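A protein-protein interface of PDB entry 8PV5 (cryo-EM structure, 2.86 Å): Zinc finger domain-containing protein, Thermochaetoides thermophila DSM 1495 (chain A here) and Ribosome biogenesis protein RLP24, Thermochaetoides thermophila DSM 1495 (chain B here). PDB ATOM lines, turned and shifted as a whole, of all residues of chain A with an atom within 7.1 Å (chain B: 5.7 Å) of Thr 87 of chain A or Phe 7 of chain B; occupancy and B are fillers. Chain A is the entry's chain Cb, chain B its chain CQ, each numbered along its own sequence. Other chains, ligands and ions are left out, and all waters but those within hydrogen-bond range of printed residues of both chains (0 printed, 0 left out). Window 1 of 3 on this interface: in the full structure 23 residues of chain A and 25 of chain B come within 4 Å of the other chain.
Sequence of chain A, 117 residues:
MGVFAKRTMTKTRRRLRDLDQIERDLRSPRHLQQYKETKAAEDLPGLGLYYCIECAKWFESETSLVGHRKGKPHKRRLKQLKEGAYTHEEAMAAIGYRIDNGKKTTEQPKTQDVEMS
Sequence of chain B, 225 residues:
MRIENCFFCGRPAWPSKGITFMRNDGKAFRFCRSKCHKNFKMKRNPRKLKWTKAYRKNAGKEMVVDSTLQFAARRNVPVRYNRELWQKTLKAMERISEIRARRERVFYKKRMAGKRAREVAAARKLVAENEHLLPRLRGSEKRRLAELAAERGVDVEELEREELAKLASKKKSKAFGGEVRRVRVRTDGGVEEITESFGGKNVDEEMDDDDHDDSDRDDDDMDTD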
ATOM      1  N   ASP A  20       7.076 -23.659 -11.112  1.00  0.00           N
ATOM      2  CA  ASP A  20       5.890 -24.054 -11.866  1.00  0.00           C
ATOM      3  C   ASP A  20       5.382 -25.418 -11.421  1.00  0.00           C
ATOM      4  O   ASP A  20       4.168 -25.631 -11.328  1.00  0.00           O
ATOM      5  CB  ASP A  20       6.184 -24.038 -13.367  1.00  0.00           C
ATOM      6  CG  ASP A  20       7.524 -24.655 -13.714  1.00  0.00           C
ATOM      7  OD1 ASP A  20       8.076 -24.309 -14.780  1.00  0.00           O
ATOM      8  OD2 ASP A  20       8.024 -25.490 -12.936  1.00  0.00           O
ATOM      9  N   GLU A  23       3.472 -24.909  -8.445  1.00  0.00           N
ATOM     10  CA  GLU A  23       2.147 -24.400  -8.802  1.00  0.00           C
ATOM     11  C   GLU A  23       1.191 -25.528  -9.190  1.00  0.00           C
ATOM     12  O   GLU A  23       0.025 -25.535  -8.774  1.00  0.00           O
ATOM     13  CB  GLU A  23       2.260 -23.381  -9.936  1.00  0.00           C
ATOM     14  CG  GLU A  23       2.954 -22.089  -9.550  1.00  0.00           C
ATOM     15  CD  GLU A  23       2.475 -20.907 -10.369  1.00  0.00           C
ATOM     16  OE1 GLU A  23       2.434 -21.024 -11.611  1.00  0.00           O
ATOM     17  OE2 GLU A  23       2.138 -19.864  -9.772  1.00  0.00           O
ATOM     18  N   ARG A  24       1.664 -26.490  -9.992  1.00  0.00           N
ATOM     19  CA  ARG A  24       0.812 -27.637 -10.322  1.00  0.00           C
ATOM     20  C   ARG A  24       0.521 -28.490  -9.094  1.00  0.00           C
ATOM     21  O   ARG A  24      -0.571 -29.059  -8.976  1.00  0.00           O
ATOM     22  CB  ARG A  24       1.415 -28.519 -11.421  1.00  0.00           C
ATOM     23  CG  ARG A  24       2.333 -27.860 -12.404  1.00  0.00           C
ATOM     24  CD  ARG A  24       2.457 -28.664 -13.687  1.00  0.00           C
ATOM     25  NE  ARG A  24       1.168 -28.932 -14.314  1.00  0.00           N
ATOM     26  CZ  ARG A  24       0.507 -28.067 -15.072  1.00  0.00           C
ATOM     27  NH1 ARG A  24       0.975 -26.853 -15.307  1.00  0.00           N
ATOM     28  NH2 ARG A  24      -0.654 -28.433 -15.609  1.00  0.00           N
ATOM     29  N   GLY A  84       3.834 -15.207  -9.857  1.00  0.00           N
ATOM     30  CA  GLY A  84       3.526 -16.116 -10.942  1.00  0.00           C
ATOM     31  C   GLY A  84       4.744 -16.776 -11.553  1.00  0.00           C
ATOM     32  O   GLY A  84       5.682 -16.096 -11.982  1.00  0.00           O
ATOM     33  N   ALA A  85       4.735 -18.105 -11.604  1.00  0.00           N
ATOM     34  CA  ALA A  85       5.855 -18.846 -12.162  1.00  0.00           C
ATOM     35  C   ALA A  85       5.885 -18.721 -13.681  1.00  0.00           C
ATOM     36  O   ALA A  85       4.870 -18.454 -14.329  1.00  0.00           O
ATOM     37  CB  ALA A  85       5.773 -20.316 -11.762  1.00  0.00           C
ATOM     38  N   TYR A  86       7.071 -18.923 -14.246  1.00  0.00           N
ATOM     39  CA  TYR A  86       7.260 -18.807 -15.683  1.00  0.00           C
ATOM     40  C   TYR A  86       6.966 -20.131 -16.374  1.00  0.00           C
ATOM     41  O   TYR A  86       7.520 -21.174 -16.015  1.00  0.00           O
ATOM     42  CB  TYR A  86       8.687 -18.366 -15.990  1.00  0.00           C
ATOM     43  CG  TYR A  86       8.865 -17.808 -17.373  1.00  0.00           C
ATOM     44  CD1 TYR A  86       9.689 -18.439 -18.292  1.00  0.00           C
ATOM     45  CD2 TYR A  86       8.210 -16.649 -17.763  1.00  0.00           C
ATOM     46  CE1 TYR A  86       9.860 -17.930 -19.557  1.00  0.00           C
ATOM     47  CE2 TYR A  86       8.372 -16.136 -19.028  1.00  0.00           C
ATOM     48  CZ  TYR A  86       9.202 -16.780 -19.921  1.00  0.00           C
ATOM     49  OH  TYR A  86       9.374 -16.271 -21.185  1.00  0.00           O
ATOM     50  N   THR A  87       6.094 -20.084 -17.378  1.00  0.00           N
ATOM     51  CA  THR A  87       5.640 -21.273 -18.081  1.00  0.00           C
ATOM     52  C   THR A  87       5.855 -21.103 -19.580  1.00  0.00           C
ATOM     53  O   THR A  87       6.220 -20.026 -20.070  1.00  0.00           O
ATOM     54  CB  THR A  87       4.163 -21.565 -17.783  1.00  0.00           C
ATOM     55  OG1 THR A  87       3.378 -20.400 -18.067  1.00  0.00           O
ATOM     56  CG2 THR A  87       3.972 -21.962 -16.327  1.00  0.00           C
ATOM     57  N   HIS A  88       5.617 -22.195 -20.314  1.00  0.00           N
ATOM     58  CA  HIS A  88       5.741 -22.165 -21.766  1.00  0.00           C
ATOM     59  C   HIS A  88       4.660 -21.307 -22.405  1.00  0.00           C
ATOM     60  O   HIS A  88       4.892 -20.720 -23.465  1.00  0.00           O
ATOM     61  CB  HIS A  88       5.694 -23.583 -22.331  1.00  0.00           C
ATOM     62  CG  HIS A  88       7.013 -24.287 -22.302  1.00  0.00           C
ATOM     63  ND1 HIS A  88       7.394 -25.113 -21.268  1.00  0.00           N
ATOM     64  CD2 HIS A  88       8.044 -24.284 -23.180  1.00  0.00           C
ATOM     65  CE1 HIS A  88       8.601 -25.594 -21.511  1.00  0.00           C
ATOM     66  NE2 HIS A  88       9.018 -25.104 -22.665  1.00  0.00           N
ATOM     67  N   GLU A  89       3.483 -21.216 -21.780  1.00  0.00           N
ATOM     68  CA  GLU A  89       2.447 -20.313 -22.275  1.00  0.00           C
ATOM     69  C   GLU A  89       2.893 -18.858 -22.182  1.00  0.00           C
ATOM     70  O   GLU A  89       2.671 -18.077 -23.114  1.00  0.00           O
ATOM     71  CB  GLU A  89       1.144 -20.526 -21.501  1.00  0.00           C
ATOM     72  CG  GLU A  89       0.475 -21.878 -21.730  1.00  0.00           C
ATOM     73  CD  GLU A  89       1.055 -22.992 -20.875  1.00  0.00           C
ATOM     74  OE1 GLU A  89       1.947 -22.711 -20.048  1.00  0.00           O
ATOM     75  OE2 GLU A  89       0.620 -24.151 -21.035  1.00  0.00           O
ATOM     76  N   GLU A  90       3.540 -18.483 -21.076  1.00  0.00           N
ATOM     77  CA  GLU A  90       4.070 -17.130 -20.949  1.00  0.00           C
ATOM     78  C   GLU A  90       5.224 -16.892 -21.915  1.00  0.00           C
ATOM     79  O   GLU A  90       5.342 -15.803 -22.490  1.00  0.00           O
ATOM     80  CB  GLU A  90       4.512 -16.869 -19.511  1.00  0.00           C
ATOM     81  CG  GLU A  90       3.375 -16.865 -18.506  1.00  0.00           C
ATOM     82  CD  GLU A  90       3.725 -16.115 -17.239  1.00  0.00           C
ATOM     83  OE1 GLU A  90       4.265 -14.994 -17.343  1.00  0.00           O
ATOM     84  OE2 GLU A  90       3.458 -16.644 -16.140  1.00  0.00           O
ATOM     85  N   ALA A  91       6.076 -17.903 -22.113  1.00  0.00           N
ATOM     86  CA  ALA A  91       7.174 -17.771 -23.069  1.00  0.00           C
ATOM     87  C   ALA A  91       6.657 -17.618 -24.494  1.00  0.00           C
ATOM     88  O   ALA A  91       7.256 -16.910 -25.310  1.00  0.00           O
ATOM     89  CB  ALA A  91       8.106 -18.976 -22.964  1.00  0.00           C
ATOM     90  N   MET A  92       5.543 -18.280 -24.808  1.00  0.00           N
ATOM     91  CA  MET A  92       4.951 -18.175 -26.136  1.00  0.00           C
ATOM     92  C   MET A  92       4.240 -16.836 -26.319  1.00  0.00           C
ATOM     93  O   MET A  92       4.294 -16.231 -27.398  1.00  0.00           O
ATOM     94  CB  MET A  92       3.999 -19.354 -26.339  1.00  0.00           C
ATOM     95  CG  MET A  92       3.264 -19.387 -27.651  1.00  0.00           C
ATOM     96  SD  MET A  92       2.475 -20.974 -27.998  1.00  0.00           S
ATOM     97  CE  MET A  92       2.168 -21.598 -26.348  1.00  0.00           C
ATOM     98  N   ALA A  93       3.582 -16.347 -25.265  1.00  0.00           N
ATOM     99  CA  ALA A  93       2.937 -15.041 -25.336  1.00  0.00           C
ATOM    100  C   ALA A  93       3.954 -13.910 -25.407  1.00  0.00           C
ATOM    101  O   ALA A  93       3.646 -12.836 -25.935  1.00  0.00           O
ATOM    102  CB  ALA A  93       2.012 -14.844 -24.137  1.00  0.00           C
ATOM    103  N   ASN B   5      12.075 -21.470 -30.511  1.00  0.00           N
ATOM    104  CA  ASN B   5      12.319 -20.251 -29.758  1.00  0.00           C
ATOM    105  C   ASN B   5      12.827 -20.610 -28.372  1.00  0.00           C
ATOM    106  O   ASN B   5      12.424 -21.621 -27.789  1.00  0.00           O
ATOM    107  CB  ASN B   5      11.063 -19.387 -29.662  1.00  0.00           C
ATOM    108  CG  ASN B   5      10.821 -18.577 -30.917  1.00  0.00           C
ATOM    109  OD1 ASN B   5      11.216 -17.416 -31.005  1.00  0.00           O
ATOM    110  ND2 ASN B   5      10.169 -19.187 -31.899  1.00  0.00           N
ATOM    111  N   CYS B   6      13.731 -19.779 -27.860  1.00  0.00           N
ATOM    112  CA  CYS B   6      14.306 -20.008 -26.544  1.00  0.00           C
ATOM    113  C   CYS B   6      13.245 -19.840 -25.467  1.00  0.00           C
ATOM    114  O   CYS B   6      12.434 -18.912 -25.509  1.00  0.00           O
ATOM    115  CB  CYS B   6      15.467 -19.045 -26.296  1.00  0.00           C
ATOM    116  SG  CYS B   6      16.280 -19.234 -24.692  1.00  0.00           S
ATOM    117  N   PHE B   7      13.237 -20.769 -24.511  1.00  0.00           N
ATOM    118  CA  PHE B   7      12.275 -20.696 -23.420  1.00  0.00           C
ATOM    119  C   PHE B   7      12.560 -19.504 -22.516  1.00  0.00           C
ATOM    120  O   PHE B   7      11.633 -18.885 -21.985  1.00  0.00           O
ATOM    121  CB  PHE B   7      12.294 -21.999 -22.623  1.00  0.00           C
ATOM    122  CG  PHE B   7      11.491 -21.952 -21.357  1.00  0.00           C
ATOM    123  CD1 PHE B   7      10.109 -21.992 -21.400  1.00  0.00           C
ATOM    124  CD2 PHE B   7      12.119 -21.880 -20.125  1.00  0.00           C
ATOM    125  CE1 PHE B   7       9.367 -21.950 -20.238  1.00  0.00           C
ATOM    126  CE2 PHE B   7      11.382 -21.837 -18.960  1.00  0.00           C
ATOM    127  CZ  PHE B   7      10.006 -21.876 -19.016  1.00  0.00           C
ATOM    128  N   PHE B   8      13.835 -19.160 -22.349  1.00  0.00           N
ATOM    129  CA  PHE B   8      14.215 -18.143 -21.377  1.00  0.00           C
ATOM    130  C   PHE B   8      14.102 -16.735 -21.952  1.00  0.00           C
ATOM    131  O   PHE B   8      13.447 -15.870 -21.364  1.00  0.00           O
ATOM    132  CB  PHE B   8      15.635 -18.413 -20.883  1.00  0.00           C
ATOM    133  CG  PHE B   8      15.901 -17.906 -19.499  1.00  0.00           C
ATOM    134  CD1 PHE B   8      16.384 -16.625 -19.299  1.00  0.00           C
ATOM    135  CD2 PHE B   8      15.662 -18.708 -18.398  1.00  0.00           C
ATOM    136  CE1 PHE B   8      16.626 -16.155 -18.029  1.00  0.00           C
ATOM    137  CE2 PHE B   8      15.905 -18.244 -17.125  1.00  0.00           C
ATOM    138  CZ  PHE B   8      16.384 -16.964 -16.941  1.00  0.00           C
ATOM    139  N   CYS B   9      14.733 -16.485 -23.099  1.00  0.00           N
ATOM    140  CA  CYS B   9      14.815 -15.140 -23.649  1.00  0.00           C
ATOM    141  C   CYS B   9      14.025 -14.940 -24.935  1.00  0.00           C
ATOM    142  O   CYS B   9      13.876 -13.793 -25.372  1.00  0.00           O
ATOM    143  CB  CYS B   9      16.281 -14.761 -23.894  1.00  0.00           C
ATOM    144  SG  CYS B   9      17.020 -15.555 -25.326  1.00  0.00           S
ATOM    145  N   GLY B  10      13.522 -16.006 -25.555  1.00  0.00           N
ATOM    146  CA  GLY B  10      12.676 -15.881 -26.720  1.00  0.00           C
ATOM    147  C   GLY B  10      13.393 -15.675 -28.037  1.00  0.00           C
ATOM    148  O   GLY B  10      12.728 -15.422 -29.049  1.00  0.00           O
ATOM    149  N   PHE B  29      12.541 -28.112 -22.215  1.00  0.00           N
ATOM    150  CA  PHE B  29      12.927 -26.707 -22.131  1.00  0.00           C
ATOM    151  C   PHE B  29      14.081 -26.472 -23.093  1.00  0.00           C
ATOM    152  O   PHE B  29      15.167 -27.022 -22.905  1.00  0.00           O
ATOM    153  CB  PHE B  29      13.331 -26.327 -20.706  1.00  0.00           C
ATOM    154  CG  PHE B  29      12.215 -26.429 -19.710  1.00  0.00           C
ATOM    155  CD1 PHE B  29      11.939 -27.627 -19.078  1.00  0.00           C
ATOM    156  CD2 PHE B  29      11.445 -25.323 -19.408  1.00  0.00           C
ATOM    157  CE1 PHE B  29      10.912 -27.718 -18.163  1.00  0.00           C
ATOM    158  CE2 PHE B  29      10.419 -25.408 -18.495  1.00  0.00           C
ATOM    159  CZ  PHE B  29      10.152 -26.606 -17.873  1.00  0.00           C
ATOM    160  N   ARG B  30      13.858 -25.650 -24.111  1.00  0.00           N
ATOM    161  CA  ARG B  30      14.891 -25.357 -25.093  1.00  0.00           C
ATOM    162  C   ARG B  30      15.519 -24.003 -24.789  1.00  0.00           C
ATOM    163  O   ARG B  30      14.812 -23.000 -24.650  1.00  0.00           O
ATOM    164  CB  ARG B  30      14.307 -25.370 -26.504  1.00  0.00           C
ATOM    165  CG  ARG B  30      15.264 -24.897 -27.577  1.00  0.00           C
ATOM    166  CD  ARG B  30      16.392 -25.891 -27.772  1.00  0.00           C
ATOM    167  NE  ARG B  30      17.317 -25.476 -28.818  1.00  0.00           N
ATOM    168  CZ  ARG B  30      17.129 -25.691 -30.112  1.00  0.00           C
ATOM    169  NH1 ARG B  30      16.053 -26.316 -30.561  1.00  0.00           N
ATOM    170  NH2 ARG B  30      18.045 -25.270 -30.979  1.00  0.00           N
ATOM    171  N   PHE B  31      16.845 -23.977 -24.681  1.00  0.00           N
ATOM    172  CA  PHE B  31      17.597 -22.758 -24.439  1.00  0.00           C
ATOM    173  C   PHE B  31      18.538 -22.508 -25.605  1.00  0.00           C
ATOM    174  O   PHE B  31      19.191 -23.428 -26.102  1.00  0.00           O
ATOM    175  CB  PHE B  31      18.402 -22.846 -23.141  1.00  0.00           C
ATOM    176  CG  PHE B  31      17.600 -23.303 -21.968  1.00  0.00           C
ATOM    177  CD1 PHE B  31      16.696 -22.453 -21.360  1.00  0.00           C
ATOM    178  CD2 PHE B  31      17.745 -24.587 -21.474  1.00  0.00           C
ATOM    179  CE1 PHE B  31      15.953 -22.873 -20.285  1.00  0.00           C
ATOM    180  CE2 PHE B  31      17.005 -25.012 -20.398  1.00  0.00           C
ATOM    181  CZ  PHE B  31      16.107 -24.154 -19.805  1.00  0.00           C
ATOM    182  N   CYS B  32      18.602 -21.251 -26.033  1.00  0.00           N
ATOM    183  CA  CYS B  32      19.430 -20.870 -27.164  1.00  0.00           C
ATOM    184  C   CYS B  32      20.909 -20.758 -26.821  1.00  0.00           C
ATOM    185  O   CYS B  32      21.740 -20.810 -27.734  1.00  0.00           O
ATOM    186  CB  CYS B  32      18.948 -19.536 -27.740  1.00  0.00           C
ATOM    187  SG  CYS B  32      19.333 -18.112 -26.703  1.00  0.00           S
ATOM    188  N   PHE B  40      18.621 -20.364 -15.966  1.00  0.00           N
ATOM    189  CA  PHE B  40      17.547 -21.289 -15.616  1.00  0.00           C
ATOM    190  C   PHE B  40      17.971 -22.232 -14.495  1.00  0.00           C
ATOM    191  O   PHE B  40      17.185 -22.509 -13.581  1.00  0.00           O
ATOM    192  CB  PHE B  40      17.116 -22.079 -16.854  1.00  0.00           C
ATOM    193  CG  PHE B  40      15.972 -23.027 -16.610  1.00  0.00           C
ATOM    194  CD1 PHE B  40      14.665 -22.579 -16.668  1.00  0.00           C
ATOM    195  CD2 PHE B  40      16.203 -24.369 -16.343  1.00  0.00           C
ATOM    196  CE1 PHE B  40      13.612 -23.444 -16.449  1.00  0.00           C
ATOM    197  CE2 PHE B  40      15.154 -25.235 -16.121  1.00  0.00           C
ATOM    198  CZ  PHE B  40      13.859 -24.773 -16.175  1.00  0.00           C
ATOM    199  N   PRO B  46      12.890 -15.229 -15.766  1.00  0.00           N
ATOM    200  CA  PRO B  46      13.068 -14.439 -16.997  1.00  0.00           C
ATOM    201  C   PRO B  46      12.267 -13.150 -17.025  1.00  0.00           C
ATOM    202  O   PRO B  46      12.662 -12.194 -17.701  1.00  0.00           O
ATOM    203  CB  PRO B  46      12.606 -15.407 -18.096  1.00  0.00           C
ATOM    204  CG  PRO B  46      12.710 -16.754 -17.495  1.00  0.00           C
ATOM    205  CD  PRO B  46      12.392 -16.583 -16.047  1.00  0.00           C
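N of Phe 7 of chain B is in hydrogen-bond range of O of Arg 30 of chain B (2.7 Å). The side-chain hydroxyl (OG1) of Thr 87 of chain A lies within hydrogen-bond range of the side-chain carboxylate (OE1) of Glu 89 of chain A (3.4 Å).
Among the printed residues, pairs that only touch across the chains: Tyr 86 of chain A with Phe 7 of chain B, His 88 of chain A with Phe 29 of chain B, His 88 of chain A with Phe 7 of chain B, Tyr 86 of chain A with Pro 46 of chain B, Ala 91 of chain A with Phe 7 of chain B and Thr 87 of chain A with Phe 7 of chain B.
Thr 87 of chain A touches just one residue of chain B: Phe 7. Of the printed residues of chain B, Ala 91 of chain A touches Phe 7. Of the printed residues of chain A, Phe 29 of chain B touches His 88 (3.5 Å). Printed residues of chain B within 4 Å of His 88 of chain A: Phe 7 (3.5 Å) and Phe 29 (3.5 Å). Printed residues of chain B within 4 Å of Tyr 86 of chain A: Phe 7 (3.2 Å) and Pro 46 (3.5 Å). Asn 5 of chain B touches none of the printed residues of chain A. Met 92 of chain A touches none of the printed residues of chain B. The nearest printed residue of chain B that does not touch Thr 87 of chain A is Phe 29 of chain B (6.3 Å). The nearest printed residue of chain B that does not touch Ala 91 of chain A is Cys 6 of chain B (5.0 Å).
Of the 12 printed residues of chain B, 3 touch a printed residue of chain A. Printed residues of chain B that touch a printed residue of chain A: Phe 7, Phe 29 and Pro 46. Among the printed residues, no Asp or Glu carboxylate lies within 4 Å of a Lys or Arg side-chain nitrogen of the other chain.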
